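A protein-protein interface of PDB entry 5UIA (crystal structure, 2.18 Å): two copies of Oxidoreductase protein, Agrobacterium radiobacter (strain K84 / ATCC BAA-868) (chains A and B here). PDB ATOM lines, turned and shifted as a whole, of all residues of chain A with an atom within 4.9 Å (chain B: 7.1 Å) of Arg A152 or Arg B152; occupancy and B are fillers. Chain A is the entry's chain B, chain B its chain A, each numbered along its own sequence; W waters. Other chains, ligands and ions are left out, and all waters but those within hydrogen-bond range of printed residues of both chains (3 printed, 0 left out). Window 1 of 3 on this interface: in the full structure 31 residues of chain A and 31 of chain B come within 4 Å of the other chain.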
ATOM      1  N   TRP A 150      -7.682  -6.320   1.196  1.00  0.00           N
ATOM      2  CA  TRP A 150      -6.862  -5.774   2.267  1.00  0.00           C
ATOM      3  C   TRP A 150      -7.754  -5.169   3.334  1.00  0.00           C
ATOM      4  O   TRP A 150      -8.780  -4.586   3.003  1.00  0.00           O
ATOM      5  CB  TRP A 150      -5.888  -4.707   1.719  1.00  0.00           C
ATOM      6  CG  TRP A 150      -4.930  -4.212   2.747  1.00  0.00           C
ATOM      7  CD1 TRP A 150      -3.770  -4.809   3.136  1.00  0.00           C
ATOM      8  CD2 TRP A 150      -5.071  -3.040   3.554  1.00  0.00           C
ATOM      9  NE1 TRP A 150      -3.171  -4.079   4.135  1.00  0.00           N
ATOM     10  CE2 TRP A 150      -3.946  -2.984   4.408  1.00  0.00           C
ATOM     11  CE3 TRP A 150      -6.024  -2.015   3.623  1.00  0.00           C
ATOM     12  CZ2 TRP A 150      -3.753  -1.949   5.325  1.00  0.00           C
ATOM     13  CZ3 TRP A 150      -5.834  -0.988   4.544  1.00  0.00           C
ATOM     14  CH2 TRP A 150      -4.710  -0.965   5.377  1.00  0.00           C
ATOM     15  N   GLY A 151      -7.344  -5.290   4.600  1.00  0.00           N
ATOM     16  CA  GLY A 151      -8.054  -4.672   5.716  1.00  0.00           C
ATOM     17  C   GLY A 151      -7.166  -4.202   6.867  1.00  0.00           C
ATOM     18  O   GLY A 151      -6.065  -4.725   7.089  1.00  0.00           O
ATOM     19  N   ARG A 152      -7.637  -3.183   7.583  1.00  0.00           N
ATOM     20  CA  ARG A 152      -7.062  -2.805   8.870  1.00  0.00           C
ATOM     21  C   ARG A 152      -8.176  -2.761   9.895  1.00  0.00           C
ATOM     22  O   ARG A 152      -9.220  -2.183   9.620  1.00  0.00           O
ATOM     23  CB  ARG A 152      -6.385  -1.442   8.810  1.00  0.00           C
ATOM     24  CG  ARG A 152      -5.568  -1.142  10.059  1.00  0.00           C
ATOM     25  CD  ARG A 152      -5.205   0.321  10.147  1.00  0.00           C
ATOM     26  NE  ARG A 152      -4.534   0.635  11.407  1.00  0.00           N
ATOM     27  CZ  ARG A 152      -4.364   1.863  11.886  1.00  0.00           C
ATOM     28  NH1 ARG A 152      -4.797   2.926  11.219  1.00  0.00           N
ATOM     29  NH2 ARG A 152      -3.757   2.039  13.046  1.00  0.00           N
ATOM     30  N   PHE A 153      -7.938  -3.371  11.059  1.00  0.00           N
ATOM     31  CA  PHE A 153      -8.865  -3.345  12.194  1.00  0.00           C
ATOM     32  C   PHE A 153      -8.110  -2.814  13.427  1.00  0.00           C
ATOM     33  O   PHE A 153      -7.191  -3.455  13.909  1.00  0.00           O
ATOM     34  CB  PHE A 153      -9.420  -4.753  12.443  1.00  0.00           C
ATOM     35  CG  PHE A 153      -9.991  -5.409  11.207  1.00  0.00           C
ATOM     36  CD1 PHE A 153      -9.175  -6.141  10.345  1.00  0.00           C
ATOM     37  CD2 PHE A 153     -11.338  -5.277  10.891  1.00  0.00           C
ATOM     38  CE1 PHE A 153      -9.699  -6.729   9.201  1.00  0.00           C
ATOM     39  CE2 PHE A 153     -11.866  -5.862   9.753  1.00  0.00           C
ATOM     40  CZ  PHE A 153     -11.045  -6.591   8.904  1.00  0.00           C
ATOM     41  N   SER A 154      -8.511  -1.650  13.930  1.00  0.00           N
ATOM     42  CA  SER A 154      -7.684  -0.860  14.825  1.00  0.00           C
ATOM     43  C   SER A 154      -8.461  -0.403  16.060  1.00  0.00           C
ATOM     44  O   SER A 154      -9.528   0.181  15.937  1.00  0.00           O
ATOM     45  CB  SER A 154      -7.172   0.363  14.061  1.00  0.00           C
ATOM     46  OG  SER A 154      -6.176   1.064  14.790  1.00  0.00           O
ATOM     47  N   ARG A 156      -7.101   1.715  19.246  1.00  0.00           N
ATOM     48  CA  ARG A 156      -5.990   2.404  19.896  1.00  0.00           C
ATOM     49  C   ARG A 156      -6.568   3.403  20.885  1.00  0.00           C
ATOM     50  O   ARG A 156      -7.215   4.366  20.482  1.00  0.00           O
ATOM     51  CB  ARG A 156      -5.109   3.113  18.856  1.00  0.00           C
ATOM     52  CG  ARG A 156      -4.616   2.194  17.747  1.00  0.00           C
ATOM     53  CD  ARG A 156      -3.427   2.775  16.994  1.00  0.00           C
ATOM     54  NE  ARG A 156      -2.177   2.637  17.742  1.00  0.00           N
ATOM     55  CZ  ARG A 156      -1.470   1.508  17.887  1.00  0.00           C
ATOM     56  NH1 ARG A 156      -1.864   0.354  17.345  1.00  0.00           N
ATOM     57  NH2 ARG A 156      -0.341   1.532  18.597  1.00  0.00           N
ATOM     58  N   SER A 226      -4.732  -8.680   6.259  1.00  0.00           N
ATOM     59  CA  SER A 226      -5.166  -7.627   7.183  1.00  0.00           C
ATOM     60  C   SER A 226      -4.178  -7.331   8.312  1.00  0.00           C
ATOM     61  O   SER A 226      -3.296  -8.140   8.638  1.00  0.00           O
ATOM     62  CB  SER A 226      -6.545  -7.925   7.768  1.00  0.00           C
ATOM     63  OG  SER A 226      -6.480  -8.947   8.737  1.00  0.00           O
ATOM     64  N   ILE A 227      -4.342  -6.143   8.881  1.00  0.00           N
ATOM     65  CA  ILE A 227      -3.581  -5.689  10.020  1.00  0.00           C
ATOM     66  C   ILE A 227      -4.563  -5.557  11.164  1.00  0.00           C
ATOM     67  O   ILE A 227      -5.584  -4.909  11.013  1.00  0.00           O
ATOM     68  CB  ILE A 227      -2.928  -4.317   9.730  1.00  0.00           C
ATOM     69  CG1 ILE A 227      -1.859  -4.451   8.636  1.00  0.00           C
ATOM     70  CG2 ILE A 227      -2.327  -3.693  10.990  1.00  0.00           C
ATOM     71  CD1 ILE A 227      -0.711  -5.376   8.975  1.00  0.00           C
ATOM     72  N   ASP A 229      -4.248  -4.043  14.836  1.00  0.00           N
ATOM     73  CA  ASP A 229      -3.391  -3.308  15.759  1.00  0.00           C
ATOM     74  C   ASP A 229      -4.231  -2.811  16.930  1.00  0.00           C
ATOM     75  O   ASP A 229      -5.272  -2.188  16.730  1.00  0.00           O
ATOM     76  CB  ASP A 229      -2.655  -2.166  15.049  1.00  0.00           C
ATOM     77  CG  ASP A 229      -3.586  -1.128  14.473  1.00  0.00           C
ATOM     78  OD1 ASP A 229      -4.118  -1.355  13.366  1.00  0.00           O
ATOM     79  OD2 ASP A 229      -3.771  -0.074  15.119  1.00  0.00           O
ATOM     80  N   LEU A 245     -11.887   0.940  14.577  1.00  0.00           N
ATOM     81  CA  LEU A 245     -11.781   1.627  13.281  1.00  0.00           C
ATOM     82  C   LEU A 245     -11.374   0.624  12.210  1.00  0.00           C
ATOM     83  O   LEU A 245     -10.455  -0.154  12.420  1.00  0.00           O
ATOM     84  CB  LEU A 245     -10.789   2.789  13.390  1.00  0.00           C
ATOM     85  CG  LEU A 245     -11.035   3.714  14.602  1.00  0.00           C
ATOM     86  CD1 LEU A 245     -10.107   4.912  14.583  1.00  0.00           C
ATOM     87  CD2 LEU A 245     -12.490   4.167  14.693  1.00  0.00           C
ATOM     88  N   ILE A 246     -12.081   0.630  11.081  1.00  0.00           N
ATOM     89  CA  ILE A 246     -11.970  -0.431  10.078  1.00  0.00           C
ATOM     90  C   ILE A 246     -11.765   0.177   8.718  1.00  0.00           C
ATOM     91  O   ILE A 246     -12.544   1.024   8.309  1.00  0.00           O
ATOM     92  CB  ILE A 246     -13.237  -1.317  10.023  1.00  0.00           C
ATOM     93  CG1 ILE A 246     -13.499  -1.930  11.402  1.00  0.00           C
ATOM     94  CG2 ILE A 246     -13.097  -2.418   8.964  1.00  0.00           C
ATOM     95  CD1 ILE A 246     -14.690  -2.862  11.485  1.00  0.00           C
ATOM     96  N   ASP A 247     -10.718  -0.274   8.026  1.00  0.00           N
ATOM     97  CA  ASP A 247     -10.492   0.046   6.612  1.00  0.00           C
ATOM     98  C   ASP A 247     -10.529  -1.255   5.804  1.00  0.00           C
ATOM     99  O   ASP A 247      -9.910  -2.229   6.194  1.00  0.00           O
ATOM    100  CB  ASP A 247      -9.139   0.736   6.414  1.00  0.00           C
ATOM    101  CG  ASP A 247      -8.982   1.990   7.266  1.00  0.00           C
ATOM    102  OD1 ASP A 247      -9.977   2.477   7.857  1.00  0.00           O
ATOM    103  OD2 ASP A 247      -7.845   2.490   7.349  1.00  0.00           O
ATOM    104  N   TRP B 150       5.463   2.746  18.350  1.00  0.00           N
ATOM    105  CA  TRP B 150       4.673   2.163  17.258  1.00  0.00           C
ATOM    106  C   TRP B 150       4.463   3.176  16.147  1.00  0.00           C
ATOM    107  O   TRP B 150       4.228   4.357  16.415  1.00  0.00           O
ATOM    108  CB  TRP B 150       3.303   1.697  17.769  1.00  0.00           C
ATOM    109  CG  TRP B 150       2.454   1.024  16.724  1.00  0.00           C
ATOM    110  CD1 TRP B 150       2.471  -0.302  16.370  1.00  0.00           C
ATOM    111  CD2 TRP B 150       1.463   1.647  15.898  1.00  0.00           C
ATOM    112  NE1 TRP B 150       1.556  -0.532  15.367  1.00  0.00           N
ATOM    113  CE2 TRP B 150       0.919   0.643  15.067  1.00  0.00           C
ATOM    114  CE3 TRP B 150       0.972   2.957  15.788  1.00  0.00           C
ATOM    115  CZ2 TRP B 150      -0.078   0.911  14.132  1.00  0.00           C
ATOM    116  CZ3 TRP B 150      -0.023   3.220  14.860  1.00  0.00           C
ATOM    117  CH2 TRP B 150      -0.535   2.202  14.043  1.00  0.00           C
ATOM    118  N   GLY B 151       4.508   2.709  14.902  1.00  0.00           N
ATOM    119  CA  GLY B 151       4.191   3.563  13.764  1.00  0.00           C
ATOM    120  C   GLY B 151       3.392   2.904  12.651  1.00  0.00           C
ATOM    121  O   GLY B 151       3.395   1.683  12.505  1.00  0.00           O
ATOM    122  N   ARG B 152       2.714   3.736  11.863  1.00  0.00           N
ATOM    123  CA  ARG B 152       2.136   3.321  10.590  1.00  0.00           C
ATOM    124  C   ARG B 152       2.513   4.327   9.510  1.00  0.00           C
ATOM    125  O   ARG B 152       2.301   5.535   9.687  1.00  0.00           O
ATOM    126  CB  ARG B 152       0.616   3.232  10.665  1.00  0.00           C
ATOM    127  CG  ARG B 152       0.006   2.635   9.408  1.00  0.00           C
ATOM    128  CD  ARG B 152      -1.443   3.010   9.200  1.00  0.00           C
ATOM    129  NE  ARG B 152      -1.912   2.448   7.933  1.00  0.00           N
ATOM    130  CZ  ARG B 152      -3.148   2.548   7.451  1.00  0.00           C
ATOM    131  NH1 ARG B 152      -4.105   3.183   8.122  1.00  0.00           N
ATOM    132  NH2 ARG B 152      -3.428   2.001   6.281  1.00  0.00           N
ATOM    133  N   PHE B 153       3.028   3.811   8.393  1.00  0.00           N
ATOM    134  CA  PHE B 153       3.399   4.612   7.235  1.00  0.00           C
ATOM    135  C   PHE B 153       2.615   4.118   6.013  1.00  0.00           C
ATOM    136  O   PHE B 153       2.862   3.023   5.527  1.00  0.00           O
ATOM    137  CB  PHE B 153       4.900   4.487   6.989  1.00  0.00           C
ATOM    138  CG  PHE B 153       5.739   4.860   8.179  1.00  0.00           C
ATOM    139  CD1 PHE B 153       6.140   6.176   8.378  1.00  0.00           C
ATOM    140  CD2 PHE B 153       6.121   3.900   9.112  1.00  0.00           C
ATOM    141  CE1 PHE B 153       6.912   6.532   9.476  1.00  0.00           C
ATOM    142  CE2 PHE B 153       6.893   4.249  10.214  1.00  0.00           C
ATOM    143  CZ  PHE B 153       7.285   5.568  10.397  1.00  0.00           C
ATOM    144  N   SER B 154       1.697   4.938   5.506  1.00  0.00           N
ATOM    145  CA  SER B 154       0.714   4.487   4.512  1.00  0.00           C
ATOM    146  C   SER B 154       0.691   5.330   3.226  1.00  0.00           C
ATOM    147  O   SER B 154       0.635   6.557   3.272  1.00  0.00           O
ATOM    148  CB  SER B 154      -0.680   4.506   5.150  1.00  0.00           C
ATOM    149  OG  SER B 154      -1.571   3.675   4.435  1.00  0.00           O
ATOM    150  N   PHE B 155       0.729   4.656   2.082  1.00  0.00           N
ATOM    151  CA  PHE B 155       0.517   5.283   0.781  1.00  0.00           C
ATOM    152  C   PHE B 155      -0.425   4.349   0.037  1.00  0.00           C
ATOM    153  O   PHE B 155       0.009   3.333  -0.504  1.00  0.00           O
ATOM    154  CB  PHE B 155       1.861   5.443   0.056  1.00  0.00           C
ATOM    155  CG  PHE B 155       1.803   6.265  -1.215  1.00  0.00           C
ATOM    156  CD1 PHE B 155       1.168   5.787  -2.363  1.00  0.00           C
ATOM    157  CD2 PHE B 155       2.445   7.507  -1.284  1.00  0.00           C
ATOM    158  CE1 PHE B 155       1.145   6.537  -3.529  1.00  0.00           C
ATOM    159  CE2 PHE B 155       2.427   8.253  -2.451  1.00  0.00           C
ATOM    160  CZ  PHE B 155       1.779   7.768  -3.575  1.00  0.00           C
ATOM    161  N   ARG B 156      -1.713   4.677   0.057  1.00  0.00           N
ATOM    162  CA  ARG B 156      -2.753   3.923  -0.650  1.00  0.00           C
ATOM    163  C   ARG B 156      -3.405   4.857  -1.671  1.00  0.00           C
ATOM    164  O   ARG B 156      -3.937   5.912  -1.312  1.00  0.00           O
ATOM    165  CB  ARG B 156      -3.790   3.347   0.329  1.00  0.00           C
ATOM    166  CG  ARG B 156      -3.170   2.608   1.521  1.00  0.00           C
ATOM    167  CD  ARG B 156      -4.189   1.787   2.310  1.00  0.00           C
ATOM    168  NE  ARG B 156      -4.538   0.549   1.600  1.00  0.00           N
ATOM    169  CZ  ARG B 156      -3.779  -0.546   1.548  1.00  0.00           C
ATOM    170  NH1 ARG B 156      -2.603  -0.618   2.180  1.00  0.00           N
ATOM    171  NH2 ARG B 156      -4.198  -1.590   0.844  1.00  0.00           N
ATOM    172  N   THR B 183       8.590   4.560   1.121  1.00  0.00           N
ATOM    173  CA  THR B 183       7.846   4.434   2.382  1.00  0.00           C
ATOM    174  C   THR B 183       8.719   3.779   3.450  1.00  0.00           C
ATOM    175  O   THR B 183       8.678   4.163   4.622  1.00  0.00           O
ATOM    176  CB  THR B 183       6.540   3.630   2.197  1.00  0.00           C
ATOM    177  OG1 THR B 183       5.958   3.929   0.928  1.00  0.00           O
ATOM    178  CG2 THR B 183       5.527   3.974   3.292  1.00  0.00           C
ATOM    179  N   LEU B 191      11.836   6.241  12.501  1.00  0.00           N
ATOM    180  CA  LEU B 191      11.936   5.296  13.630  1.00  0.00           C
ATOM    181  C   LEU B 191      13.255   4.529  13.729  1.00  0.00           C
ATOM    182  O   LEU B 191      13.403   3.685  14.615  1.00  0.00           O
ATOM    183  CB  LEU B 191      10.760   4.306  13.588  1.00  0.00           C
ATOM    184  CG  LEU B 191       9.366   4.895  13.805  1.00  0.00           C
ATOM    185  CD1 LEU B 191       8.316   3.799  13.737  1.00  0.00           C
ATOM    186  CD2 LEU B 191       9.279   5.628  15.132  1.00  0.00           C
ATOM    187  N   THR B 225       7.765  -1.082  16.755  1.00  0.00           N
ATOM    188  CA  THR B 225       7.097  -1.832  15.697  1.00  0.00           C
ATOM    189  C   THR B 225       6.456  -0.827  14.750  1.00  0.00           C
ATOM    190  O   THR B 225       5.821   0.126  15.207  1.00  0.00           O
ATOM    191  CB  THR B 225       5.981  -2.729  16.265  1.00  0.00           C
ATOM    192  OG1 THR B 225       6.500  -3.514  17.335  1.00  0.00           O
ATOM    193  CG2 THR B 225       5.439  -3.667  15.199  1.00  0.00           C
ATOM    194  N   SER B 226       6.626  -1.024  13.443  1.00  0.00           N
ATOM    195  CA  SER B 226       5.885  -0.231  12.465  1.00  0.00           C
ATOM    196  C   SER B 226       5.232  -1.078  11.364  1.00  0.00           C
ATOM    197  O   SER B 226       5.619  -2.227  11.117  1.00  0.00           O
ATOM    198  CB  SER B 226       6.764   0.882  11.865  1.00  0.00           C
ATOM    199  OG  SER B 226       7.639   0.380  10.872  1.00  0.00           O
ATOM    200  N   ILE B 227       4.212  -0.490  10.749  1.00  0.00           N
ATOM    201  CA  ILE B 227       3.523  -1.053   9.592  1.00  0.00           C
ATOM    202  C   ILE B 227       3.805  -0.142   8.412  1.00  0.00           C
ATOM    203  O   ILE B 227       3.580   1.063   8.499  1.00  0.00           O
ATOM    204  CB  ILE B 227       1.997  -1.089   9.802  1.00  0.00           C
ATOM    205  CG1 ILE B 227       1.620  -2.038  10.948  1.00  0.00           C
ATOM    206  CG2 ILE B 227       1.272  -1.488   8.518  1.00  0.00           C
ATOM    207  CD1 ILE B 227       1.961  -3.492  10.692  1.00  0.00           C
ATOM    208  N   VAL B 228       4.293  -0.717   7.317  1.00  0.00           N
ATOM    209  CA  VAL B 228       4.391  -0.011   6.037  1.00  0.00           C
ATOM    210  C   VAL B 228       3.416  -0.684   5.066  1.00  0.00           C
ATOM    211  O   VAL B 228       3.565  -1.864   4.741  1.00  0.00           O
ATOM    212  CB  VAL B 228       5.831  -0.016   5.492  1.00  0.00           C
ATOM    213  CG1 VAL B 228       5.880   0.582   4.103  1.00  0.00           C
ATOM    214  CG2 VAL B 228       6.743   0.755   6.434  1.00  0.00           C
ATOM    215  N   ASP B 229       2.403   0.055   4.633  1.00  0.00           N
ATOM    216  CA  ASP B 229       1.398  -0.497   3.742  1.00  0.00           C
ATOM    217  C   ASP B 229       1.242   0.409   2.526  1.00  0.00           C
ATOM    218  O   ASP B 229       1.029   1.609   2.658  1.00  0.00           O
ATOM    219  CB  ASP B 229       0.064  -0.728   4.473  1.00  0.00           C
ATOM    220  CG  ASP B 229      -0.559   0.550   5.009  1.00  0.00           C
ATOM    221  OD1 ASP B 229      -0.111   1.055   6.057  1.00  0.00           O
ATOM    222  OD2 ASP B 229      -1.521   1.045   4.392  1.00  0.00           O
ATOM    223  N   THR B 244       1.899  10.625   1.791  1.00  0.00           N
ATOM    224  CA  THR B 244       2.188   9.510   2.672  1.00  0.00           C
ATOM    225  C   THR B 244       1.603   9.882   4.046  1.00  0.00           C
ATOM    226  O   THR B 244       1.904  10.944   4.595  1.00  0.00           O
ATOM    227  CB  THR B 244       3.701   9.217   2.753  1.00  0.00           C
ATOM    228  OG1 THR B 244       4.219   8.889   1.449  1.00  0.00           O
ATOM    229  CG2 THR B 244       3.977   8.049   3.706  1.00  0.00           C
ATOM    230  N   LEU B 245       0.735   9.019   4.569  1.00  0.00           N
ATOM    231  CA  LEU B 245       0.046   9.257   5.837  1.00  0.00           C
ATOM    232  C   LEU B 245       0.772   8.508   6.953  1.00  0.00           C
ATOM    233  O   LEU B 245       1.146   7.351   6.787  1.00  0.00           O
ATOM    234  CB  LEU B 245      -1.417   8.814   5.724  1.00  0.00           C
ATOM    235  CG  LEU B 245      -2.151   9.398   4.508  1.00  0.00           C
ATOM    236  CD1 LEU B 245      -3.595   8.913   4.451  1.00  0.00           C
ATOM    237  CD2 LEU B 245      -2.085  10.925   4.529  1.00  0.00           C
ATOM    238  N   ILE B 246       0.989   9.184   8.077  1.00  0.00           N
ATOM    239  CA  ILE B 246       1.876   8.683   9.128  1.00  0.00           C
ATOM    240  C   ILE B 246       1.193   8.755  10.490  1.00  0.00           C
ATOM    241  O   ILE B 246       0.697   9.813  10.879  1.00  0.00           O
ATOM    242  CB  ILE B 246       3.211   9.463   9.153  1.00  0.00           C
ATOM    243  CG1 ILE B 246       3.918   9.288   7.802  1.00  0.00           C
ATOM    244  CG2 ILE B 246       4.097   8.977  10.307  1.00  0.00           C
ATOM    245  CD1 ILE B 246       5.219  10.023   7.658  1.00  0.00           C
ATOM    246  N   ASP B 247       1.146   7.625  11.191  1.00  0.00           N
ATOM    247  CA  ASP B 247       0.768   7.595  12.614  1.00  0.00           C
ATOM    248  C   ASP B 247       1.975   7.167  13.457  1.00  0.00           C
ATOM    249  O   ASP B 247       2.609   6.169  13.141  1.00  0.00           O
ATOM    250  CB  ASP B 247      -0.378   6.607  12.875  1.00  0.00           C
ATOM    251  CG  ASP B 247      -1.629   6.887  12.041  1.00  0.00           C
ATOM    252  OD1 ASP B 247      -1.788   7.974  11.441  1.00  0.00           O
ATOM    253  OD2 ASP B 247      -2.462   5.979  11.989  1.00  0.00           O
ATOM    254  N   ILE B 248       2.281   7.910  14.520  1.00  0.00           N
ATOM    255  CA  ILE B 248       3.341   7.536  15.471  1.00  0.00           C
ATOM    256  C   ILE B 248       2.766   7.589  16.880  1.00  0.00           C
ATOM    257  O   ILE B 248       2.143   8.579  17.254  1.00  0.00           O
ATOM    258  CB  ILE B 248       4.560   8.486  15.415  1.00  0.00           C
ATOM    259  CG1 ILE B 248       5.051   8.728  13.978  1.00  0.00           C
ATOM    260  CG2 ILE B 248       5.705   7.953  16.286  1.00  0.00           C
ATOM    261  CD1 ILE B 248       5.699   7.528  13.319  1.00  0.00           C
ATOM    262  N   ASP B 249       2.960   6.528  17.657  1.00  0.00           N
ATOM    263  CA  ASP B 249       2.578   6.529  19.071  1.00  0.00           C
ATOM    264  C   ASP B 249       3.856   6.542  19.912  1.00  0.00           C
ATOM    265  O   ASP B 249       4.777   5.765  19.658  1.00  0.00           O
ATOM    266  CB  ASP B 249       1.742   5.296  19.427  1.00  0.00           C
ATOM    267  CG  ASP B 249       0.339   5.307  18.802  1.00  0.00           C
ATOM    268  OD1 ASP B 249       0.011   6.236  18.012  1.00  0.00           O
ATOM    269  OD2 ASP B 249      -0.438   4.362  19.128  1.00  0.00           O
ATOM    270  N   ARG B 256      -0.187  12.380  14.307  1.00  0.00           N
ATOM    271  CA  ARG B 256      -1.091  11.934  13.237  1.00  0.00           C
ATOM    272  C   ARG B 256      -0.982  12.907  12.072  1.00  0.00           C
ATOM    273  O   ARG B 256      -1.434  14.056  12.165  1.00  0.00           O
ATOM    274  CB  ARG B 256      -2.535  11.840  13.748  1.00  0.00           C
ATOM    275  CG  ARG B 256      -2.755  10.764  14.818  1.00  0.00           C
ATOM    276  CD  ARG B 256      -2.622   9.358  14.240  1.00  0.00           C
ATOM    277  NE  ARG B 256      -2.983   8.308  15.201  1.00  0.00           N
ATOM    278  CZ  ARG B 256      -2.164   7.771  16.114  1.00  0.00           C
ATOM    279  NH1 ARG B 256      -0.891   8.176  16.249  1.00  0.00           N
ATOM    280  NH2 ARG B 256      -2.628   6.815  16.914  1.00  0.00           N
ATOM    281  N   LEU B 257      -0.324  12.458  11.002  1.00  0.00           N
ATOM    282  CA  LEU B 257      -0.280  13.184   9.743  1.00  0.00           C
ATOM    283  C   LEU B 257      -1.342  12.546   8.857  1.00  0.00           C
ATOM    284  O   LEU B 257      -1.193  11.406   8.432  1.00  0.00           O
ATOM    285  CB  LEU B 257       1.118  13.088   9.107  1.00  0.00           C
ATOM    286  CG  LEU B 257       1.327  13.657   7.701  1.00  0.00           C
ATOM    287  CD1 LEU B 257       1.122  15.159   7.682  1.00  0.00           C
ATOM    288  CD2 LEU B 257       2.716  13.317   7.204  1.00  0.00           C
HETATM  289  O   HOH W   1      -1.116  -3.054   1.631  1.00  0.00           O
HETATM  290  O   HOH W   2      -6.920   3.669   9.483  1.00  0.00           O
HETATM  291  O   HOH W   3      -0.338  -1.901  17.899  1.00  0.00           O
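NH1 of Arg A152 lies within salt-bridge range of OD2 of Asp B247 (3.9 Å). The guanidinium group (NE) of Arg A156 lies within salt-bridge range of the side-chain carboxylate (OD2) of Asp B249 (2.8 Å). The guanidinium group (NH1) of Arg B152 sits close to the guanidinium group (NH1) of Arg A152 (3.2 Å). NH1 of Arg B152 is in salt-bridge range of OD2 of Asp A247, at 3.9 Å.
Of the printed residues of chain B, Arg A152 touches Trp B150 (3.4 Å), Arg B152 (3.2 Å) and Asp B247 (3.9 Å). Of chain A, only Trp A150, Arg A152 and Asp A247 come within 4 Å of Arg B152. Of the printed residues of chain B, Ile A227 touches Ile B227 (3.7 Å). Of the printed residues of chain B, Trp A150 touches Arg B152, Arg B156 and Asp B229. Of the printed residues of chain A, Trp B150 touches Arg A152, Arg A156 and Asp A229. Of the printed residues of chain A, Arg B156 touches Trp A150. Thr B244 touches none of the printed residues of chain A. The nearest printed residue of chain A that does not touch Arg B152 is Asp A229 (6.6 Å).
Water W2 lies within hydrogen-bond range of OD2 of Asp A247 (2.6 Å), NH1 of Arg A152 (2.8 Å) and NH1 of Arg B152 (3.2 Å). Water W3 lies within hydrogen-bond range of NH1 of Arg A156 (2.8 Å) and NE1 of Trp B150 (3.4 Å). Water W1 bridges NH1 of Arg B156 (2.9 Å) and NE1 of Trp A150 (3.4 Å).
Among the printed residues, pairs that only touch across the chains: Trp A150 with Arg B156, Arg A156 with Trp B150, Trp A150 with Arg B152, Arg A152 with Trp B150, Ile A227 with Ile B227, Trp A150 with Asp B229 and Asp A229 with Trp B150.
Trp A150 touches Arg B156, and with the chains exchanged Arg A156 touches Trp B150. Arg A152 touches its own counterpart, Arg B152. Arg A152 touches Asp B247, and with the chains exchanged Asp A247 touches Arg B152. Ile A227 touches its own counterpart, Ile B227. 12 positions are printed for both chains. Of the 11 pairs that touch across the chains among the printed residues, 10 have their exchanged pair printed and touching as well.
N of Phe A153 is in hydrogen-bond range of O of Ile A227 (2.8 Å). The backbone carbonyl oxygen of Phe B153 is in hydrogen-bond range of the backbone NH of Asp B229 (3.1 Å). The side-chain hydroxyl of Ser B154 is in hydrogen-bond range of the guanidinium group of Arg B152, 3.1 Å away. The side-chain hydroxyl (OG) of Ser B154 lies within hydrogen-bond range of the side-chain carboxylate (OD2) of Asp B229 (2.6 Å). The side-chain carboxylate (OD2) of Asp A229 sits at hydrogen-bond distance from the side-chain hydroxyl (OG) of Ser A154 (2.7 Å). The backbone carbonyl oxygen of Gly A151 is in hydrogen-bond range of the backbone NH of Ile A227 (2.9 Å).
Hydrophobic or aromatic side chains of chain A within 4 Å of the printed part of chain B: Trp A150 and Ile A227. Among the printed residues, Asp or Glu carboxylates within 4 Å of a Lys or Arg side-chain nitrogen of the other chain: Arg A152 with Asp B247, Arg A156 with Asp B249 and Asp A247 with Arg B152.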
